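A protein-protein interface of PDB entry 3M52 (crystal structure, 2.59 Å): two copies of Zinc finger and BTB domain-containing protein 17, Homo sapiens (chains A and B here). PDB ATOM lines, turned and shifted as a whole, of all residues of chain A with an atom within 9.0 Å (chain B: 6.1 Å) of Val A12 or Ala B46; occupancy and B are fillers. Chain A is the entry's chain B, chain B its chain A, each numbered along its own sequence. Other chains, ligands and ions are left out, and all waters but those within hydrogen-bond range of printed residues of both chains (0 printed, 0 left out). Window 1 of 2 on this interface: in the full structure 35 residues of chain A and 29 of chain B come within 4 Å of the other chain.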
ATOM      1  N   PHE A   5      -4.643  -3.449 -12.594  1.00  0.00           N
ATOM      2  CA  PHE A   5      -4.975  -4.704 -11.910  1.00  0.00           C
ATOM      3  C   PHE A   5      -4.177  -5.875 -12.511  1.00  0.00           C
ATOM      4  O   PHE A   5      -4.759  -6.713 -13.210  1.00  0.00           O
ATOM      5  N   PRO A   6      -2.853  -5.951 -12.219  1.00  0.00           N
ATOM      6  CA  PRO A   6      -1.934  -6.882 -12.904  1.00  0.00           C
ATOM      7  C   PRO A   6      -2.218  -8.375 -12.677  1.00  0.00           C
ATOM      8  O   PRO A   6      -1.773  -9.209 -13.475  1.00  0.00           O
ATOM      9  CB  PRO A   6      -0.559  -6.505 -12.337  1.00  0.00           C
ATOM     10  CG  PRO A   6      -0.854  -5.909 -11.014  1.00  0.00           C
ATOM     11  CD  PRO A   6      -2.148  -5.163 -11.191  1.00  0.00           C
ATOM     12  N   GLN A   7      -2.952  -8.704 -11.613  1.00  0.00           N
ATOM     13  CA  GLN A   7      -3.379 -10.086 -11.361  1.00  0.00           C
ATOM     14  C   GLN A   7      -4.292 -10.612 -12.475  1.00  0.00           C
ATOM     15  O   GLN A   7      -4.435 -11.820 -12.650  1.00  0.00           O
ATOM     16  CB  GLN A   7      -4.069 -10.208  -9.997  1.00  0.00           C
ATOM     17  N   HIS A   8      -4.901  -9.699 -13.228  1.00  0.00           N
ATOM     18  CA  HIS A   8      -5.796 -10.073 -14.323  1.00  0.00           C
ATOM     19  C   HIS A   8      -5.059 -10.777 -15.482  1.00  0.00           C
ATOM     20  O   HIS A   8      -5.653 -11.605 -16.170  1.00  0.00           O
ATOM     21  CB  HIS A   8      -6.611  -8.863 -14.793  1.00  0.00           C
ATOM     22  CG  HIS A   8      -7.327  -9.080 -16.087  1.00  0.00           C
ATOM     23  ND1 HIS A   8      -8.474  -9.838 -16.187  1.00  0.00           N
ATOM     24  CD2 HIS A   8      -7.055  -8.639 -17.337  1.00  0.00           C
ATOM     25  CE1 HIS A   8      -8.880  -9.852 -17.444  1.00  0.00           C
ATOM     26  NE2 HIS A   8      -8.033  -9.134 -18.162  1.00  0.00           N
ATOM     27  N   SER A   9      -3.779 -10.453 -15.681  1.00  0.00           N
ATOM     28  CA  SER A   9      -2.907 -11.185 -16.618  1.00  0.00           C
ATOM     29  C   SER A   9      -2.899 -12.675 -16.283  1.00  0.00           C
ATOM     30  O   SER A   9      -3.212 -13.520 -17.129  1.00  0.00           O
ATOM     31  CB  SER A   9      -1.461 -10.677 -16.552  1.00  0.00           C
ATOM     32  OG  SER A   9      -1.371  -9.268 -16.664  1.00  0.00           O
ATOM     33  N   GLN A  10      -2.549 -12.972 -15.032  1.00  0.00           N
ATOM     34  CA  GLN A  10      -2.507 -14.337 -14.505  1.00  0.00           C
ATOM     35  C   GLN A  10      -3.830 -15.046 -14.692  1.00  0.00           C
ATOM     36  O   GLN A  10      -3.860 -16.258 -14.862  1.00  0.00           O
ATOM     37  CB  GLN A  10      -2.154 -14.331 -13.020  1.00  0.00           C
ATOM     38  CG  GLN A  10      -0.786 -13.783 -12.701  1.00  0.00           C
ATOM     39  CD  GLN A  10      -0.573 -13.617 -11.217  1.00  0.00           C
ATOM     40  OE1 GLN A  10      -0.677 -14.581 -10.452  1.00  0.00           O
ATOM     41  NE2 GLN A  10      -0.270 -12.395 -10.794  1.00  0.00           N
ATOM     42  N   HIS A  11      -4.918 -14.284 -14.642  1.00  0.00           N
ATOM     43  CA  HIS A  11      -6.265 -14.811 -14.854  1.00  0.00           C
ATOM     44  C   HIS A  11      -6.488 -15.216 -16.320  1.00  0.00           C
ATOM     45  O   HIS A  11      -7.083 -16.264 -16.598  1.00  0.00           O
ATOM     46  CB  HIS A  11      -7.304 -13.784 -14.372  1.00  0.00           C
ATOM     47  CG  HIS A  11      -8.707 -14.067 -14.814  1.00  0.00           C
ATOM     48  ND1 HIS A  11      -9.553 -13.076 -15.271  1.00  0.00           N
ATOM     49  CD2 HIS A  11      -9.413 -15.221 -14.861  1.00  0.00           C
ATOM     50  CE1 HIS A  11     -10.717 -13.616 -15.596  1.00  0.00           C
ATOM     51  NE2 HIS A  11     -10.657 -14.915 -15.357  1.00  0.00           N
ATOM     52  N   VAL A  12      -5.990 -14.399 -17.248  1.00  0.00           N
ATOM     53  CA  VAL A  12      -6.174 -14.654 -18.680  1.00  0.00           C
ATOM     54  C   VAL A  12      -5.404 -15.901 -19.150  1.00  0.00           C
ATOM     55  O   VAL A  12      -5.979 -16.779 -19.803  1.00  0.00           O
ATOM     56  CB  VAL A  12      -5.814 -13.422 -19.547  1.00  0.00           C
ATOM     57  CG1 VAL A  12      -6.103 -13.704 -21.004  1.00  0.00           C
ATOM     58  CG2 VAL A  12      -6.602 -12.201 -19.098  1.00  0.00           C
ATOM     59  N   LEU A  13      -4.121 -15.980 -18.797  1.00  0.00           N
ATOM     60  CA  LEU A  13      -3.278 -17.112 -19.184  1.00  0.00           C
ATOM     61  C   LEU A  13      -3.679 -18.418 -18.478  1.00  0.00           C
ATOM     62  O   LEU A  13      -3.660 -19.491 -19.106  1.00  0.00           O
ATOM     63  CB  LEU A  13      -1.796 -16.792 -18.966  1.00  0.00           C
ATOM     64  CG  LEU A  13      -0.729 -17.727 -19.548  1.00  0.00           C
ATOM     65  CD1 LEU A  13      -0.725 -17.718 -21.058  1.00  0.00           C
ATOM     66  CD2 LEU A  13       0.635 -17.333 -19.028  1.00  0.00           C
ATOM     67  N   GLU A  14      -4.044 -18.326 -17.194  1.00  0.00           N
ATOM     68  CA  GLU A  14      -4.575 -19.479 -16.450  1.00  0.00           C
ATOM     69  C   GLU A  14      -5.788 -20.080 -17.147  1.00  0.00           C
ATOM     70  O   GLU A  14      -5.895 -21.293 -17.270  1.00  0.00           O
ATOM     71  CB  GLU A  14      -4.962 -19.098 -15.020  1.00  0.00           C
ATOM     72  CG  GLU A  14      -3.867 -19.299 -13.984  1.00  0.00           C
ATOM     73  CD  GLU A  14      -4.266 -18.808 -12.587  1.00  0.00           C
ATOM     74  OE1 GLU A  14      -5.478 -18.601 -12.334  1.00  0.00           O
ATOM     75  OE2 GLU A  14      -3.361 -18.633 -11.733  1.00  0.00           O
ATOM     76  N   GLN A  15      -6.695 -19.218 -17.596  1.00  0.00           N
ATOM     77  CA  GLN A  15      -7.907 -19.632 -18.289  1.00  0.00           C
ATOM     78  C   GLN A  15      -7.649 -20.116 -19.711  1.00  0.00           C
ATOM     79  O   GLN A  15      -8.367 -20.972 -20.219  1.00  0.00           O
ATOM     80  CB  GLN A  15      -8.919 -18.486 -18.306  1.00  0.00           C
ATOM     81  CG  GLN A  15      -9.566 -18.224 -16.953  1.00  0.00           C
ATOM     82  CD  GLN A  15     -10.495 -19.336 -16.524  1.00  0.00           C
ATOM     83  OE1 GLN A  15     -11.269 -19.854 -17.327  1.00  0.00           O
ATOM     84  NE2 GLN A  15     -10.431 -19.704 -15.249  1.00  0.00           N
ATOM     85  N   LEU A  16      -6.639 -19.548 -20.360  1.00  0.00           N
ATOM     86  CA  LEU A  16      -6.267 -19.993 -21.692  1.00  0.00           C
ATOM     87  C   LEU A  16      -5.719 -21.411 -21.615  1.00  0.00           C
ATOM     88  O   LEU A  16      -6.002 -22.233 -22.486  1.00  0.00           O
ATOM     89  CB  LEU A  16      -5.275 -19.032 -22.337  1.00  0.00           C
ATOM     90  CG  LEU A  16      -5.845 -17.667 -22.750  1.00  0.00           C
ATOM     91  CD1 LEU A  16      -4.720 -16.662 -22.958  1.00  0.00           C
ATOM     92  CD2 LEU A  16      -6.715 -17.759 -23.994  1.00  0.00           C
ATOM     93  N   ASN A  17      -4.966 -21.699 -20.550  1.00  0.00           N
ATOM     94  CA  ASN A  17      -4.484 -23.055 -20.287  1.00  0.00           C
ATOM     95  C   ASN A  17      -5.581 -24.034 -19.891  1.00  0.00           C
ATOM     96  O   ASN A  17      -5.531 -25.205 -20.267  1.00  0.00           O
ATOM     97  CB  ASN A  17      -3.374 -23.072 -19.241  1.00  0.00           C
ATOM     98  CG  ASN A  17      -2.576 -24.365 -19.275  1.00  0.00           C
ATOM     99  OD1 ASN A  17      -2.380 -24.955 -20.337  1.00  0.00           O
ATOM    100  ND2 ASN A  17      -2.121 -24.811 -18.118  1.00  0.00           N
ATOM    101  N   GLN A  18      -6.554 -23.554 -19.124  1.00  0.00           N
ATOM    102  CA  GLN A  18      -7.774 -24.308 -18.841  1.00  0.00           C
ATOM    103  C   GLN A  18      -8.508 -24.687 -20.141  1.00  0.00           C
ATOM    104  O   GLN A  18      -8.992 -25.806 -20.268  1.00  0.00           O
ATOM    105  CB  GLN A  18      -8.682 -23.492 -17.912  1.00  0.00           C
ATOM    106  CG  GLN A  18      -9.623 -24.306 -17.028  1.00  0.00           C
ATOM    107  CD  GLN A  18     -11.118 -24.055 -17.299  1.00  0.00           C
ATOM    108  OE1 GLN A  18     -11.597 -24.196 -18.435  1.00  0.00           O
ATOM    109  NE2 GLN A  18     -11.862 -23.694 -16.243  1.00  0.00           N
ATOM    110  N   GLN A  19      -8.565 -23.757 -21.099  1.00  0.00           N
ATOM    111  CA  GLN A  19      -9.199 -23.978 -22.406  1.00  0.00           C
ATOM    112  C   GLN A  19      -8.501 -25.075 -23.213  1.00  0.00           C
ATOM    113  O   GLN A  19      -9.162 -25.913 -23.829  1.00  0.00           O
ATOM    114  CB  GLN A  19      -9.236 -22.681 -23.228  1.00  0.00           C
ATOM    115  CG  GLN A  19     -10.230 -21.639 -22.728  1.00  0.00           C
ATOM    116  CD  GLN A  19     -10.277 -20.395 -23.599  1.00  0.00           C
ATOM    117  OE1 GLN A  19      -9.967 -20.442 -24.786  1.00  0.00           O
ATOM    118  NE2 GLN A  19     -10.679 -19.273 -23.010  1.00  0.00           N
ATOM    119  N   LEU A  24     -10.831 -26.578 -25.909  1.00  0.00           N
ATOM    120  CA  LEU A  24     -11.744 -25.467 -26.188  1.00  0.00           C
ATOM    121  C   LEU A  24     -11.083 -24.289 -26.895  1.00  0.00           C
ATOM    122  O   LEU A  24     -10.070 -23.761 -26.431  1.00  0.00           O
ATOM    123  CB  LEU A  24     -12.367 -24.965 -24.882  1.00  0.00           C
ATOM    124  CG  LEU A  24     -13.817 -25.285 -24.493  1.00  0.00           C
ATOM    125  CD1 LEU A  24     -14.134 -26.777 -24.409  1.00  0.00           C
ATOM    126  CD2 LEU A  24     -14.107 -24.614 -23.163  1.00  0.00           C
ATOM    127  N   LEU A  25     -11.680 -23.880 -28.013  1.00  0.00           N
ATOM    128  CA  LEU A  25     -11.266 -22.679 -28.750  1.00  0.00           C
ATOM    129  C   LEU A  25      -9.814 -22.710 -29.234  1.00  0.00           C
ATOM    130  O   LEU A  25      -9.212 -21.669 -29.544  1.00  0.00           O
ATOM    131  CB  LEU A  25     -11.542 -21.414 -27.930  1.00  0.00           C
ATOM    132  CG  LEU A  25     -12.999 -21.195 -27.531  1.00  0.00           C
ATOM    133  CD1 LEU A  25     -13.088 -20.092 -26.505  1.00  0.00           C
ATOM    134  CD2 LEU A  25     -13.866 -20.891 -28.753  1.00  0.00           C
ATOM    135  N   HIS A  40      -3.736 -22.379 -29.022  1.00  0.00           N
ATOM    136  CA  HIS A  40      -4.284 -21.160 -29.611  1.00  0.00           C
ATOM    137  C   HIS A  40      -3.231 -20.457 -30.446  1.00  0.00           C
ATOM    138  O   HIS A  40      -2.150 -20.148 -29.946  1.00  0.00           O
ATOM    139  CB  HIS A  40      -4.759 -20.183 -28.530  1.00  0.00           C
ATOM    140  CG  HIS A  40      -5.687 -20.790 -27.529  1.00  0.00           C
ATOM    141  ND1 HIS A  40      -5.248 -21.321 -26.335  1.00  0.00           N
ATOM    142  CD2 HIS A  40      -7.028 -20.956 -27.546  1.00  0.00           C
ATOM    143  CE1 HIS A  40      -6.279 -21.796 -25.663  1.00  0.00           C
ATOM    144  NE2 HIS A  40      -7.372 -21.584 -26.374  1.00  0.00           N
ATOM    145  N   VAL A  43      -1.974 -17.275 -28.595  1.00  0.00           N
ATOM    146  CA  VAL A  43      -0.993 -17.559 -27.532  1.00  0.00           C
ATOM    147  C   VAL A  43       0.421 -17.824 -28.095  1.00  0.00           C
ATOM    148  O   VAL A  43       1.394 -17.250 -27.609  1.00  0.00           O
ATOM    149  CB  VAL A  43      -1.444 -18.743 -26.599  1.00  0.00           C
ATOM    150  CG1 VAL A  43      -0.345 -19.123 -25.619  1.00  0.00           C
ATOM    151  CG2 VAL A  43      -2.727 -18.389 -25.829  1.00  0.00           C
ATOM    152  N   MET A  79       4.859 -21.616 -22.503  1.00  0.00           N
ATOM    153  CA  MET A  79       4.021 -20.535 -23.014  1.00  0.00           C
ATOM    154  C   MET A  79       2.749 -20.345 -22.202  1.00  0.00           C
ATOM    155  O   MET A  79       2.334 -19.218 -21.953  1.00  0.00           O
ATOM    156  CB  MET A  79       3.664 -20.803 -24.468  1.00  0.00           C
ATOM    157  CG  MET A  79       4.838 -20.703 -25.407  1.00  0.00           C
ATOM    158  SD  MET A  79       4.301 -21.209 -27.035  1.00  0.00           S
ATOM    159  CE  MET A  79       5.676 -20.660 -28.054  1.00  0.00           C
ATOM    160  N   TYR A  80       2.151 -21.455 -21.777  1.00  0.00           N
ATOM    161  CA  TYR A  80       0.885 -21.427 -21.040  1.00  0.00           C
ATOM    162  C   TYR A  80       1.026 -21.313 -19.516  1.00  0.00           C
ATOM    163  O   TYR A  80       0.104 -20.851 -18.842  1.00  0.00           O
ATOM    164  CB  TYR A  80       0.037 -22.656 -21.397  1.00  0.00           C
ATOM    165  CG  TYR A  80      -0.706 -22.528 -22.708  1.00  0.00           C
ATOM    166  CD1 TYR A  80      -0.134 -22.971 -23.907  1.00  0.00           C
ATOM    167  CD2 TYR A  80      -1.979 -21.960 -22.755  1.00  0.00           C
ATOM    168  CE1 TYR A  80      -0.814 -22.851 -25.126  1.00  0.00           C
ATOM    169  CE2 TYR A  80      -2.673 -21.839 -23.959  1.00  0.00           C
ATOM    170  CZ  TYR A  80      -2.083 -22.285 -25.143  1.00  0.00           C
ATOM    171  OH  TYR A  80      -2.768 -22.165 -26.327  1.00  0.00           O
ATOM    172  N   LEU B  13      -0.134 -11.046 -22.239  1.00  0.00           N
ATOM    173  CA  LEU B  13      -1.301 -10.167 -22.352  1.00  0.00           C
ATOM    174  C   LEU B  13      -1.002  -8.926 -23.172  1.00  0.00           C
ATOM    175  O   LEU B  13      -1.775  -8.564 -24.057  1.00  0.00           O
ATOM    176  CB  LEU B  13      -1.844  -9.762 -20.976  1.00  0.00           C
ATOM    177  CG  LEU B  13      -3.081  -8.858 -20.929  1.00  0.00           C
ATOM    178  CD1 LEU B  13      -4.255  -9.454 -21.703  1.00  0.00           C
ATOM    179  CD2 LEU B  13      -3.469  -8.603 -19.492  1.00  0.00           C
ATOM    180  N   LEU B  16      -1.096  -9.829 -26.686  1.00  0.00           N
ATOM    181  CA  LEU B  16      -2.431 -10.093 -27.216  1.00  0.00           C
ATOM    182  C   LEU B  16      -3.179  -8.788 -27.516  1.00  0.00           C
ATOM    183  O   LEU B  16      -4.001  -8.730 -28.434  1.00  0.00           O
ATOM    184  CB  LEU B  16      -3.238 -11.000 -26.273  1.00  0.00           C
ATOM    185  CG  LEU B  16      -2.752 -12.460 -26.119  1.00  0.00           C
ATOM    186  CD1 LEU B  16      -3.404 -13.155 -24.929  1.00  0.00           C
ATOM    187  CD2 LEU B  16      -2.964 -13.286 -27.384  1.00  0.00           C
ATOM    188  N   LYS B  41     -11.674 -14.521 -29.691  1.00  0.00           N
ATOM    189  CA  LYS B  41     -12.627 -15.440 -29.047  1.00  0.00           C
ATOM    190  C   LYS B  41     -12.088 -16.069 -27.745  1.00  0.00           C
ATOM    191  O   LYS B  41     -12.729 -15.987 -26.705  1.00  0.00           O
ATOM    192  CB  LYS B  41     -13.004 -16.565 -30.013  1.00  0.00           C
ATOM    193  CG  LYS B  41     -14.160 -16.275 -30.948  1.00  0.00           C
ATOM    194  CD  LYS B  41     -14.467 -17.496 -31.807  1.00  0.00           C
ATOM    195  CE  LYS B  41     -15.489 -17.165 -32.887  1.00  0.00           C
ATOM    196  NZ  LYS B  41     -15.612 -18.257 -33.911  1.00  0.00           N
ATOM    197  N   ALA B  42     -10.905 -16.683 -27.821  1.00  0.00           N
ATOM    198  CA  ALA B  42     -10.251 -17.319 -26.667  1.00  0.00           C
ATOM    199  C   ALA B  42     -10.068 -16.379 -25.459  1.00  0.00           C
ATOM    200  O   ALA B  42     -10.201 -16.799 -24.306  1.00  0.00           O
ATOM    201  CB  ALA B  42      -8.904 -17.912 -27.092  1.00  0.00           C
ATOM    202  N   VAL B  43      -9.770 -15.112 -25.743  1.00  0.00           N
ATOM    203  CA  VAL B  43      -9.539 -14.093 -24.711  1.00  0.00           C
ATOM    204  C   VAL B  43     -10.821 -13.631 -24.008  1.00  0.00           C
ATOM    205  O   VAL B  43     -10.821 -13.429 -22.794  1.00  0.00           O
ATOM    206  CB  VAL B  43      -8.766 -12.869 -25.285  1.00  0.00           C
ATOM    207  CG1 VAL B  43      -8.807 -11.686 -24.321  1.00  0.00           C
ATOM    208  CG2 VAL B  43      -7.321 -13.260 -25.609  1.00  0.00           C
ATOM    209  N   LEU B  44     -11.903 -13.462 -24.765  1.00  0.00           N
ATOM    210  CA  LEU B  44     -13.194 -13.093 -24.181  1.00  0.00           C
ATOM    211  C   LEU B  44     -13.702 -14.205 -23.274  1.00  0.00           C
ATOM    212  O   LEU B  44     -14.213 -13.951 -22.173  1.00  0.00           O
ATOM    213  CB  LEU B  44     -14.217 -12.801 -25.278  1.00  0.00           C
ATOM    214  CG  LEU B  44     -13.873 -11.680 -26.258  1.00  0.00           C
ATOM    215  CD1 LEU B  44     -14.946 -11.595 -27.322  1.00  0.00           C
ATOM    216  CD2 LEU B  44     -13.697 -10.343 -25.536  1.00  0.00           C
ATOM    217  N   ALA B  45     -13.552 -15.439 -23.762  1.00  0.00           N
ATOM    218  CA  ALA B  45     -13.857 -16.643 -23.003  1.00  0.00           C
ATOM    219  C   ALA B  45     -12.974 -16.768 -21.760  1.00  0.00           C
ATOM    220  O   ALA B  45     -13.435 -17.236 -20.718  1.00  0.00           O
ATOM    221  CB  ALA B  45     -13.701 -17.850 -23.881  1.00  0.00           C
ATOM    222  N   ALA B  46     -11.714 -16.354 -21.872  1.00  0.00           N
ATOM    223  CA  ALA B  46     -10.779 -16.410 -20.747  1.00  0.00           C
ATOM    224  C   ALA B  46     -11.172 -15.420 -19.656  1.00  0.00           C
ATOM    225  O   ALA B  46     -10.909 -15.652 -18.469  1.00  0.00           O
ATOM    226  CB  ALA B  46      -9.352 -16.139 -21.219  1.00  0.00           C
ATOM    227  N   CYS B  47     -11.805 -14.322 -20.076  1.00  0.00           N
ATOM    228  CA  CYS B  47     -12.191 -13.226 -19.184  1.00  0.00           C
ATOM    229  C   CYS B  47     -13.569 -13.409 -18.577  1.00  0.00           C
ATOM    230  O   CYS B  47     -13.802 -12.985 -17.445  1.00  0.00           O
ATOM    231  CB  CYS B  47     -12.150 -11.898 -19.931  1.00  0.00           C
ATOM    232  SG  CYS B  47     -10.486 -11.330 -20.291  1.00  0.00           S
ATOM    233  N   SER B  48     -14.475 -14.042 -19.318  1.00  0.00           N
ATOM    234  CA  SER B  48     -15.870 -14.090 -18.919  1.00  0.00           C
ATOM    235  C   SER B  48     -16.551 -15.399 -19.266  1.00  0.00           C
ATOM    236  O   SER B  48     -16.472 -15.866 -20.402  1.00  0.00           O
ATOM    237  CB  SER B  48     -16.634 -12.925 -19.562  1.00  0.00           C
ATOM    238  OG  SER B  48     -18.030 -13.029 -19.333  1.00  0.00           O
ATOM    239  N   LYS B  52     -17.666 -17.206 -22.815  1.00  0.00           N
ATOM    240  CA  LYS B  52     -17.304 -18.607 -22.936  1.00  0.00           C
ATOM    241  C   LYS B  52     -18.506 -19.413 -23.408  1.00  0.00           C
ATOM    242  O   LYS B  52     -18.423 -20.148 -24.384  1.00  0.00           O
ATOM    243  CB  LYS B  52     -16.790 -19.137 -21.598  1.00  0.00           C
ATOM    244  CG  LYS B  52     -16.087 -20.486 -21.688  1.00  0.00           C
ATOM    245  CD  LYS B  52     -15.544 -20.898 -20.332  1.00  0.00           C
ATOM    246  CE  LYS B  52     -14.453 -21.937 -20.470  1.00  0.00           C
ATOM    247  NZ  LYS B  52     -13.909 -22.334 -19.143  1.00  0.00           N
ATOM    248  N   MET B  79      -9.951  -6.135 -20.334  1.00  0.00           N
ATOM    249  CA  MET B  79      -9.634  -7.499 -20.742  1.00  0.00           C
ATOM    250  C   MET B  79      -8.218  -7.639 -21.297  1.00  0.00           C
ATOM    251  O   MET B  79      -7.509  -8.593 -20.965  1.00  0.00           O
ATOM    252  CB  MET B  79     -10.636  -7.986 -21.784  1.00  0.00           C
ATOM    253  CG  MET B  79     -12.005  -8.303 -21.244  1.00  0.00           C
ATOM    254  SD  MET B  79     -13.088  -8.885 -22.558  1.00  0.00           S
ATOM    255  CE  MET B  79     -14.513  -9.399 -21.618  1.00  0.00           C
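N of Ala B46 lies close to NE2 of Gln A19. The backbone carbonyl oxygen (O) of Met B79 lies within hydrogen-bond range of a ring nitrogen (NE2) of His A8, at 2.9 Å. NZ of Lys B52 lies within hydrogen-bond range of OE1 of Gln A18 (3.1 Å). NE2 of His A11 sits at hydrogen-bond distance from O of Ala B46. O of Ala B42 is in hydrogen-bond range of NE2 of Gln A19 (2.8 Å).
The side-chain amide oxygen of Gln A19 sits at hydrogen-bond distance from a ring nitrogen (NE2) of His A40, at 3.2 Å. O of Leu A24 is in hydrogen-bond range of NE2 of His A40, 3.5 Å away. OG of Ser A9 lies within hydrogen-bond range of O of Pro A6 (3.2 Å). The backbone carbonyl oxygen (O) of Val B43 is in hydrogen-bond range of the side-chain sulfur (SG) of Cys B47 (3.3 Å). O of Gln A19 is in hydrogen-bond range of N of Leu A24, 2.7 Å away. ND1 of His A40 sits at hydrogen-bond distance from OH of Tyr A80 (2.6 Å).
Ser A9 touches Leu B13. CE1 of His A11 touches O of Cys B47 (3.7 Å). CB of Ala B46 touches O of Val A12, 3.7 Å away. O of Ala B46 touches CG of Gln A15 (3.3 Å). O of Ala B42 touches CD2 of Leu A16 (3.6 Å). Ala B45 touches Gln A19 (CB to NE2, 3.5 Å). CE of Lys B52 touches CD2 of Leu A24, 3.8 Å away. Leu A25 touches Ala B42. CB of Ala B45 touches CD1 of Leu A25, at 3.5 Å. His A40 touches Ala B42.
Of chain B, only Ala B46 (3.7 Å) comes within 4 Å of Val A12. Of the printed residues of chain B, Gln A15 touches Ala B46. Printed residues of chain B within 4 Å of Gln A18: Lys B52. Printed residues of chain B within 4 Å of Gln A19: Ala B42 (2.8 Å), Ala B45 (3.5 Å) and Ala B46 (3.3 Å). Of the printed residues of chain B, Leu A24 touches Lys B52 (3.8 Å). Of the printed residues of chain A, Ala B42 touches Leu A16, Gln A19, Leu A25 and His A40. Leu B44 touches none of the printed residues of chain A. Of chain A, only Gln A19 (3.5 Å) and Leu A25 (3.5 Å) come within 4 Å of Ala B45. Of chain A, only His A11, Val A12, Gln A15 and Gln A19 come within 4 Å of Ala B46. Of chain A, only His A8 (3.6 Å) and His A11 (3.7 Å) come within 4 Å of Cys B47.
Hydrophobic or aromatic side chains of chain B within 4 Å of the printed part of chain A: Leu B13, Ala B42, Ala B45 and Ala B46. Along chain A the printed residues that touch a printed residue of chain B span positions 8 to 40. Among the printed residues, no Asp or Glu carboxylate lies within 4 Å of a Lys or Arg side-chain nitrogen of the other chain.
Positions printed for both chains: 13, 16, 43 and 79. Of the 16 pairs that touch across the chains among the printed residues, none has its exchanged pair printed and touching as well.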
